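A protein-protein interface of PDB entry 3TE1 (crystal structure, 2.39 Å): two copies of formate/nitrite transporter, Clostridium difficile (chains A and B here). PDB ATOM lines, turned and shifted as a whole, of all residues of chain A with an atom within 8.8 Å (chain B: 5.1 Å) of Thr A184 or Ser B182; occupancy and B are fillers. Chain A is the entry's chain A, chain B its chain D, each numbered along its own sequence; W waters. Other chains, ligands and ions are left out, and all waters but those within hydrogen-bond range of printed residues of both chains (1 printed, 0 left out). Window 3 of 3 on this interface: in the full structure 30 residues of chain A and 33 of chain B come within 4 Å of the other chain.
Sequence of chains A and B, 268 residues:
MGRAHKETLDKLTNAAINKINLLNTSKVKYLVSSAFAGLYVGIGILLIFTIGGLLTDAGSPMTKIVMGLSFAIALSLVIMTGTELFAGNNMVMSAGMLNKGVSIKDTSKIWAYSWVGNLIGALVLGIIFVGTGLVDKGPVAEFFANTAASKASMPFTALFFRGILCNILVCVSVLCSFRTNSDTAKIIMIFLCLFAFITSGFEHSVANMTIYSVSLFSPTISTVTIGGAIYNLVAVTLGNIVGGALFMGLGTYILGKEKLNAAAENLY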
ATOM      1  N   SER A  76       4.857  22.071 -17.799  1.00  0.00           N
ATOM      2  CA  SER A  76       6.258  22.491 -17.902  1.00  0.00           C
ATOM      3  C   SER A  76       6.813  22.848 -16.522  1.00  0.00           C
ATOM      4  O   SER A  76       7.858  22.328 -16.133  1.00  0.00           O
ATOM      5  CB  SER A  76       6.442  23.697 -18.823  1.00  0.00           C
ATOM      6  OG  SER A  76       6.505  23.234 -20.138  1.00  0.00           O
ATOM      7  N   ILE A  79       7.051  19.513 -14.267  1.00  0.00           N
ATOM      8  CA  ILE A  79       8.172  18.633 -14.648  1.00  0.00           C
ATOM      9  C   ILE A  79       9.530  19.222 -14.254  1.00  0.00           C
ATOM     10  O   ILE A  79      10.358  18.546 -13.648  1.00  0.00           O
ATOM     11  CB  ILE A  79       8.202  18.337 -16.207  1.00  0.00           C
ATOM     12  CG1 ILE A  79       6.941  17.602 -16.670  1.00  0.00           C
ATOM     13  CG2 ILE A  79       9.447  17.562 -16.601  1.00  0.00           C
ATOM     14  CD1 ILE A  79       6.371  16.620 -15.644  1.00  0.00           C
ATOM     15  N   MET A  80       9.755  20.482 -14.632  1.00  0.00           N
ATOM     16  CA  MET A  80      11.036  21.137 -14.399  1.00  0.00           C
ATOM     17  C   MET A  80      11.324  21.412 -12.912  1.00  0.00           C
ATOM     18  O   MET A  80      12.492  21.537 -12.504  1.00  0.00           O
ATOM     19  CB  MET A  80      11.123  22.420 -15.205  1.00  0.00           C
ATOM     20  CG  MET A  80      11.039  22.159 -16.700  1.00  0.00           C
ATOM     21  SD  MET A  80      12.353  21.037 -17.291  1.00  0.00           S
ATOM     22  CE  MET A  80      13.743  22.202 -17.390  1.00  0.00           C
ATOM     23  N   THR A 180      13.557  10.378 -22.104  1.00  0.00           N
ATOM     24  CA  THR A 180      14.565  11.213 -22.757  1.00  0.00           C
ATOM     25  C   THR A 180      15.414  11.888 -21.704  1.00  0.00           C
ATOM     26  O   THR A 180      14.977  12.056 -20.553  1.00  0.00           O
ATOM     27  CB  THR A 180      13.921  12.294 -23.668  1.00  0.00           C
ATOM     28  OG1 THR A 180      14.934  13.193 -24.145  1.00  0.00           O
ATOM     29  CG2 THR A 180      12.829  13.112 -22.893  1.00  0.00           C
ATOM     30  N   ASN A 181      16.627  12.260 -22.090  1.00  0.00           N
ATOM     31  CA  ASN A 181      17.436  13.113 -21.232  1.00  0.00           C
ATOM     32  C   ASN A 181      17.414  14.621 -21.583  1.00  0.00           C
ATOM     33  O   ASN A 181      17.873  15.438 -20.787  1.00  0.00           O
ATOM     34  CB  ASN A 181      18.876  12.580 -21.093  1.00  0.00           C
ATOM     35  CG  ASN A 181      19.080  11.765 -19.803  1.00  0.00           C
ATOM     36  OD1 ASN A 181      18.962  12.301 -18.685  1.00  0.00           O
ATOM     37  ND2 ASN A 181      19.410  10.474 -19.956  1.00  0.00           N
ATOM     38  N   SER A 182      16.901  14.992 -22.757  1.00  0.00           N
ATOM     39  CA  SER A 182      16.846  16.416 -23.142  1.00  0.00           C
ATOM     40  C   SER A 182      15.668  17.122 -22.416  1.00  0.00           C
ATOM     41  O   SER A 182      14.518  16.681 -22.557  1.00  0.00           O
ATOM     42  CB  SER A 182      16.738  16.585 -24.677  1.00  0.00           C
ATOM     43  OG  SER A 182      16.353  17.910 -25.027  1.00  0.00           O
ATOM     44  N   ASP A 183      15.951  18.170 -21.628  1.00  0.00           N
ATOM     45  CA  ASP A 183      14.876  18.908 -20.961  1.00  0.00           C
ATOM     46  C   ASP A 183      14.082  19.735 -21.997  1.00  0.00           C
ATOM     47  O   ASP A 183      12.873  19.906 -21.862  1.00  0.00           O
ATOM     48  CB  ASP A 183      15.403  19.841 -19.851  1.00  0.00           C
ATOM     49  CG  ASP A 183      15.919  19.093 -18.611  1.00  0.00           C
ATOM     50  OD1 ASP A 183      15.380  18.017 -18.221  1.00  0.00           O
ATOM     51  OD2 ASP A 183      16.872  19.631 -18.001  1.00  0.00           O
ATOM     52  N   THR A 184      14.771  20.275 -23.000  1.00  0.00           N
ATOM     53  CA  THR A 184      14.103  21.007 -24.083  1.00  0.00           C
ATOM     54  C   THR A 184      13.037  20.152 -24.792  1.00  0.00           C
ATOM     55  O   THR A 184      11.940  20.622 -25.064  1.00  0.00           O
ATOM     56  CB  THR A 184      15.111  21.515 -25.148  1.00  0.00           C
ATOM     57  OG1 THR A 184      15.971  22.504 -24.555  1.00  0.00           O
ATOM     58  CG2 THR A 184      14.340  22.110 -26.354  1.00  0.00           C
ATOM     59  N   ALA A 185      13.397  18.896 -25.053  1.00  0.00           N
ATOM     60  CA  ALA A 185      12.531  17.900 -25.658  1.00  0.00           C
ATOM     61  C   ALA A 185      11.356  17.546 -24.751  1.00  0.00           C
ATOM     62  O   ALA A 185      10.221  17.360 -25.221  1.00  0.00           O
ATOM     63  CB  ALA A 185      13.358  16.620 -26.025  1.00  0.00           C
ATOM     64  N   LYS A 186      11.631  17.448 -23.453  1.00  0.00           N
ATOM     65  CA  LYS A 186      10.580  17.305 -22.439  1.00  0.00           C
ATOM     66  C   LYS A 186       9.496  18.409 -22.563  1.00  0.00           C
ATOM     67  O   LYS A 186       8.286  18.136 -22.523  1.00  0.00           O
ATOM     68  CB  LYS A 186      11.194  17.341 -21.041  1.00  0.00           C
ATOM     69  CG  LYS A 186      11.865  16.016 -20.612  1.00  0.00           C
ATOM     70  CD  LYS A 186      12.681  16.169 -19.336  1.00  0.00           C
ATOM     71  CE  LYS A 186      13.312  14.876 -18.914  1.00  0.00           C
ATOM     72  NZ  LYS A 186      14.092  15.031 -17.642  1.00  0.00           N
ATOM     73  N   ILE A 187       9.953  19.644 -22.736  1.00  0.00           N
ATOM     74  CA  ILE A 187       9.070  20.791 -22.811  1.00  0.00           C
ATOM     75  C   ILE A 187       8.284  20.800 -24.152  1.00  0.00           C
ATOM     76  O   ILE A 187       7.057  20.873 -24.158  1.00  0.00           O
ATOM     77  CB  ILE A 187       9.852  22.099 -22.579  1.00  0.00           C
ATOM     78  CG1 ILE A 187      10.463  22.105 -21.176  1.00  0.00           C
ATOM     79  CG2 ILE A 187       8.954  23.312 -22.767  1.00  0.00           C
ATOM     80  CD1 ILE A 187      11.806  22.955 -21.085  1.00  0.00           C
ATOM     81  N   ILE A 188       8.987  20.726 -25.271  1.00  0.00           N
ATOM     82  CA  ILE A 188       8.329  20.485 -26.559  1.00  0.00           C
ATOM     83  C   ILE A 188       7.239  19.422 -26.423  1.00  0.00           C
ATOM     84  O   ILE A 188       6.074  19.667 -26.762  1.00  0.00           O
ATOM     85  CB  ILE A 188       9.346  20.108 -27.598  1.00  0.00           C
ATOM     86  CG1 ILE A 188      10.250  21.326 -27.821  1.00  0.00           C
ATOM     87  CG2 ILE A 188       8.673  19.536 -28.913  1.00  0.00           C
ATOM     88  CD1 ILE A 188      11.481  21.052 -28.803  1.00  0.00           C
ATOM     89  N   MET A 189       7.588  18.273 -25.849  1.00  0.00           N
ATOM     90  CA  MET A 189       6.598  17.215 -25.730  1.00  0.00           C
ATOM     91  C   MET A 189       5.415  17.629 -24.811  1.00  0.00           C
ATOM     92  O   MET A 189       4.229  17.483 -25.157  1.00  0.00           O
ATOM     93  CB  MET A 189       7.243  15.904 -25.351  1.00  0.00           C
ATOM     94  CG  MET A 189       8.092  15.306 -26.490  1.00  0.00           C
ATOM     95  SD  MET A 189       7.202  15.139 -28.062  1.00  0.00           S
ATOM     96  CE  MET A 189       6.171  13.709 -27.620  1.00  0.00           C
ATOM     97  N   ILE A 190       5.731  18.178 -23.647  1.00  0.00           N
ATOM     98  CA  ILE A 190       4.669  18.707 -22.820  1.00  0.00           C
ATOM     99  C   ILE A 190       3.814  19.709 -23.590  1.00  0.00           C
ATOM    100  O   ILE A 190       2.593  19.649 -23.541  1.00  0.00           O
ATOM    101  CB  ILE A 190       5.194  19.379 -21.581  1.00  0.00           C
ATOM    102  CG1 ILE A 190       5.763  18.304 -20.646  1.00  0.00           C
ATOM    103  CG2 ILE A 190       4.031  20.262 -20.909  1.00  0.00           C
ATOM    104  CD1 ILE A 190       6.791  18.844 -19.675  1.00  0.00           C
ATOM    105  N   PHE A 191       4.453  20.636 -24.282  1.00  0.00           N
ATOM    106  CA  PHE A 191       3.726  21.661 -25.000  1.00  0.00           C
ATOM    107  C   PHE A 191       2.803  21.041 -26.108  1.00  0.00           C
ATOM    108  O   PHE A 191       1.679  21.463 -26.261  1.00  0.00           O
ATOM    109  CB  PHE A 191       4.760  22.659 -25.549  1.00  0.00           C
ATOM    110  CG  PHE A 191       4.395  23.269 -26.881  1.00  0.00           C
ATOM    111  CD1 PHE A 191       3.606  24.410 -26.942  1.00  0.00           C
ATOM    112  CD2 PHE A 191       4.844  22.709 -28.075  1.00  0.00           C
ATOM    113  CE1 PHE A 191       3.280  24.990 -28.142  1.00  0.00           C
ATOM    114  CE2 PHE A 191       4.520  23.311 -29.291  1.00  0.00           C
ATOM    115  CZ  PHE A 191       3.729  24.439 -29.323  1.00  0.00           C
ATOM    116  N   THR B 180      18.263  22.859 -14.259  1.00  0.00           N
ATOM    117  CA  THR B 180      18.706  22.327 -15.566  1.00  0.00           C
ATOM    118  C   THR B 180      20.122  22.776 -15.966  1.00  0.00           C
ATOM    119  O   THR B 180      20.588  23.858 -15.574  1.00  0.00           O
ATOM    120  CB  THR B 180      17.725  22.663 -16.745  1.00  0.00           C
ATOM    121  OG1 THR B 180      18.242  22.169 -17.999  1.00  0.00           O
ATOM    122  CG2 THR B 180      17.536  24.159 -16.861  1.00  0.00           C
ATOM    123  N   ASN B 181      20.791  21.923 -16.749  1.00  0.00           N
ATOM    124  CA  ASN B 181      22.082  22.233 -17.356  1.00  0.00           C
ATOM    125  C   ASN B 181      21.954  22.772 -18.801  1.00  0.00           C
ATOM    126  O   ASN B 181      22.934  23.234 -19.382  1.00  0.00           O
ATOM    127  CB  ASN B 181      23.022  21.024 -17.267  1.00  0.00           C
ATOM    128  CG  ASN B 181      23.593  20.819 -15.842  1.00  0.00           C
ATOM    129  OD1 ASN B 181      23.848  21.794 -15.116  1.00  0.00           O
ATOM    130  ND2 ASN B 181      23.778  19.548 -15.438  1.00  0.00           N
ATOM    131  N   SER B 182      20.734  22.748 -19.354  1.00  0.00           N
ATOM    132  CA  SER B 182      20.491  23.190 -20.722  1.00  0.00           C
ATOM    133  C   SER B 182      20.163  24.684 -20.787  1.00  0.00           C
ATOM    134  O   SER B 182      19.162  25.150 -20.229  1.00  0.00           O
ATOM    135  CB  SER B 182      19.372  22.343 -21.379  1.00  0.00           C
ATOM    136  OG  SER B 182      19.126  22.712 -22.728  1.00  0.00           O
ATOM    137  N   ASP B 183      21.006  25.444 -21.481  1.00  0.00           N
ATOM    138  CA  ASP B 183      20.719  26.864 -21.678  1.00  0.00           C
ATOM    139  C   ASP B 183      19.453  27.144 -22.552  1.00  0.00           C
ATOM    140  O   ASP B 183      18.763  28.151 -22.346  1.00  0.00           O
ATOM    141  CB  ASP B 183      21.954  27.615 -22.190  1.00  0.00           C
ATOM    142  CG  ASP B 183      23.049  27.806 -21.091  1.00  0.00           C
ATOM    143  OD1 ASP B 183      22.835  27.448 -19.914  1.00  0.00           O
ATOM    144  OD2 ASP B 183      24.136  28.330 -21.428  1.00  0.00           O
ATOM    145  N   THR B 184      19.191  26.290 -23.550  1.00  0.00           N
ATOM    146  CA  THR B 184      17.969  26.418 -24.334  1.00  0.00           C
ATOM    147  C   THR B 184      16.737  26.199 -23.478  1.00  0.00           C
ATOM    148  O   THR B 184      15.774  26.939 -23.593  1.00  0.00           O
ATOM    149  CB  THR B 184      17.907  25.406 -25.473  1.00  0.00           C
ATOM    150  OG1 THR B 184      18.940  25.720 -26.415  1.00  0.00           O
ATOM    151  CG2 THR B 184      16.511  25.486 -26.141  1.00  0.00           C
ATOM    152  N   ALA B 185      16.767  25.177 -22.616  1.00  0.00           N
ATOM    153  CA  ALA B 185      15.623  24.904 -21.734  1.00  0.00           C
ATOM    154  C   ALA B 185      15.438  26.005 -20.671  1.00  0.00           C
ATOM    155  O   ALA B 185      14.311  26.259 -20.193  1.00  0.00           O
ATOM    156  CB  ALA B 185      15.742  23.515 -21.080  1.00  0.00           C
ATOM    157  N   LYS B 186      16.530  26.679 -20.300  1.00  0.00           N
ATOM    158  CA  LYS B 186      16.349  27.830 -19.411  1.00  0.00           C
ATOM    159  C   LYS B 186      15.654  28.948 -20.163  1.00  0.00           C
ATOM    160  O   LYS B 186      14.860  29.695 -19.605  1.00  0.00           O
ATOM    161  CB  LYS B 186      17.646  28.363 -18.839  1.00  0.00           C
ATOM    162  CG  LYS B 186      18.494  27.337 -18.090  1.00  0.00           C
ATOM    163  CD  LYS B 186      19.913  27.909 -17.914  1.00  0.00           C
ATOM    164  CE  LYS B 186      20.766  26.989 -17.029  1.00  0.00           C
ATOM    165  NZ  LYS B 186      22.011  27.649 -16.659  1.00  0.00           N
ATOM    166  N   ILE B 188      13.564  28.655 -22.625  1.00  0.00           N
ATOM    167  CA  ILE B 188      12.156  28.359 -22.914  1.00  0.00           C
ATOM    168  C   ILE B 188      11.267  28.589 -21.674  1.00  0.00           C
ATOM    169  O   ILE B 188      10.203  29.197 -21.762  1.00  0.00           O
ATOM    170  CB  ILE B 188      11.956  26.935 -23.419  1.00  0.00           C
ATOM    171  CG1 ILE B 188      12.551  26.818 -24.829  1.00  0.00           C
ATOM    172  CG2 ILE B 188      10.432  26.590 -23.397  1.00  0.00           C
ATOM    173  CD1 ILE B 188      12.945  25.391 -25.262  1.00  0.00           C
HETATM  174  O   HOH W   1      18.580  20.246 -24.973  1.00  0.00           O
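The side-chain hydroxyl (OG1) of Thr B180 lies within hydrogen-bond range of the backbone NH (N) of Ser B182 (2.9 Å). OG of Ser A182 sits close to N of Thr A184 (3.5 Å). The side-chain hydroxyl (OG) of Ser B182 is in hydrogen-bond range of the backbone NH (N) of Ala B185 (3.4 Å). The side-chain carboxylate (OD1) of Asp A183 is in salt-bridge range of the side-chain amino group (NZ) of Lys A186 (3.3 Å).
Asp A183 touches Thr B180, but with the chains exchanged Thr A180 does not touch Asp B183 (13.9 Å). Asp A183 touches Ala B185, but with the chains exchanged Ala A185 does not touch Asp B183 (10.5 Å). Thr A184 touches Ala B185, but with the chains exchanged Ala A185 does not touch Thr B184 (7.4 Å). Thr A184 touches Ile B188, but with the chains exchanged Ile A188 does not touch Thr B184 (7.2 Å).
Water W1 lies within hydrogen-bond range of OG of Ser A182, OG of Ser B182 and OG1 of Thr A184.
Thr A184 touches just these residues of chain B: Ser B182 (3.7 Å), Thr B184 (3.4 Å), Ala B185 (3.4 Å) and Ile B188 (3.7 Å). Of chain A, only Thr A184 comes within 4 Å of Ser B182. Of the printed residues of chain A, Ile B188 touches Thr A184 (3.7 Å) and Ile A187 (3.7 Å). Of the printed residues of chain B, Ile A187 touches Ala B185 (3.98 Å) and Ile B188 (3.7 Å). Ile A79 touches none of the printed residues of chain B. The nearest residue of chain A that does not touch Ser B182 is Asp A183 (4.9 Å). The nearest printed residue of chain A that does not touch Ile B188 is Ile A188 (5.5 Å).
OG1 of Thr A184 lies within hydrogen-bond range of N of Ala B185 (3.4 Å). The side-chain hydroxyl (OG1) of Thr B180 sits at hydrogen-bond distance from the side-chain carboxylate (OD2) of Asp A183 (2.9 Å).
Among the printed residues, merely in contact across the chains: Asp A183 with Ala B185, Thr A184 with Ser B182, Thr A184 with Thr B184, Thr A184 with Ile B188, Ile A187 with Ala B185 and Ile A187 with Ile B188.
Hydrophobic or aromatic side chains of chain B that line the printed part of chain A: Ala B185 and Ile B188. Among the printed residues, no Asp or Glu carboxylate lies within 4 Å of a Lys or Arg side-chain nitrogen of the other chain.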
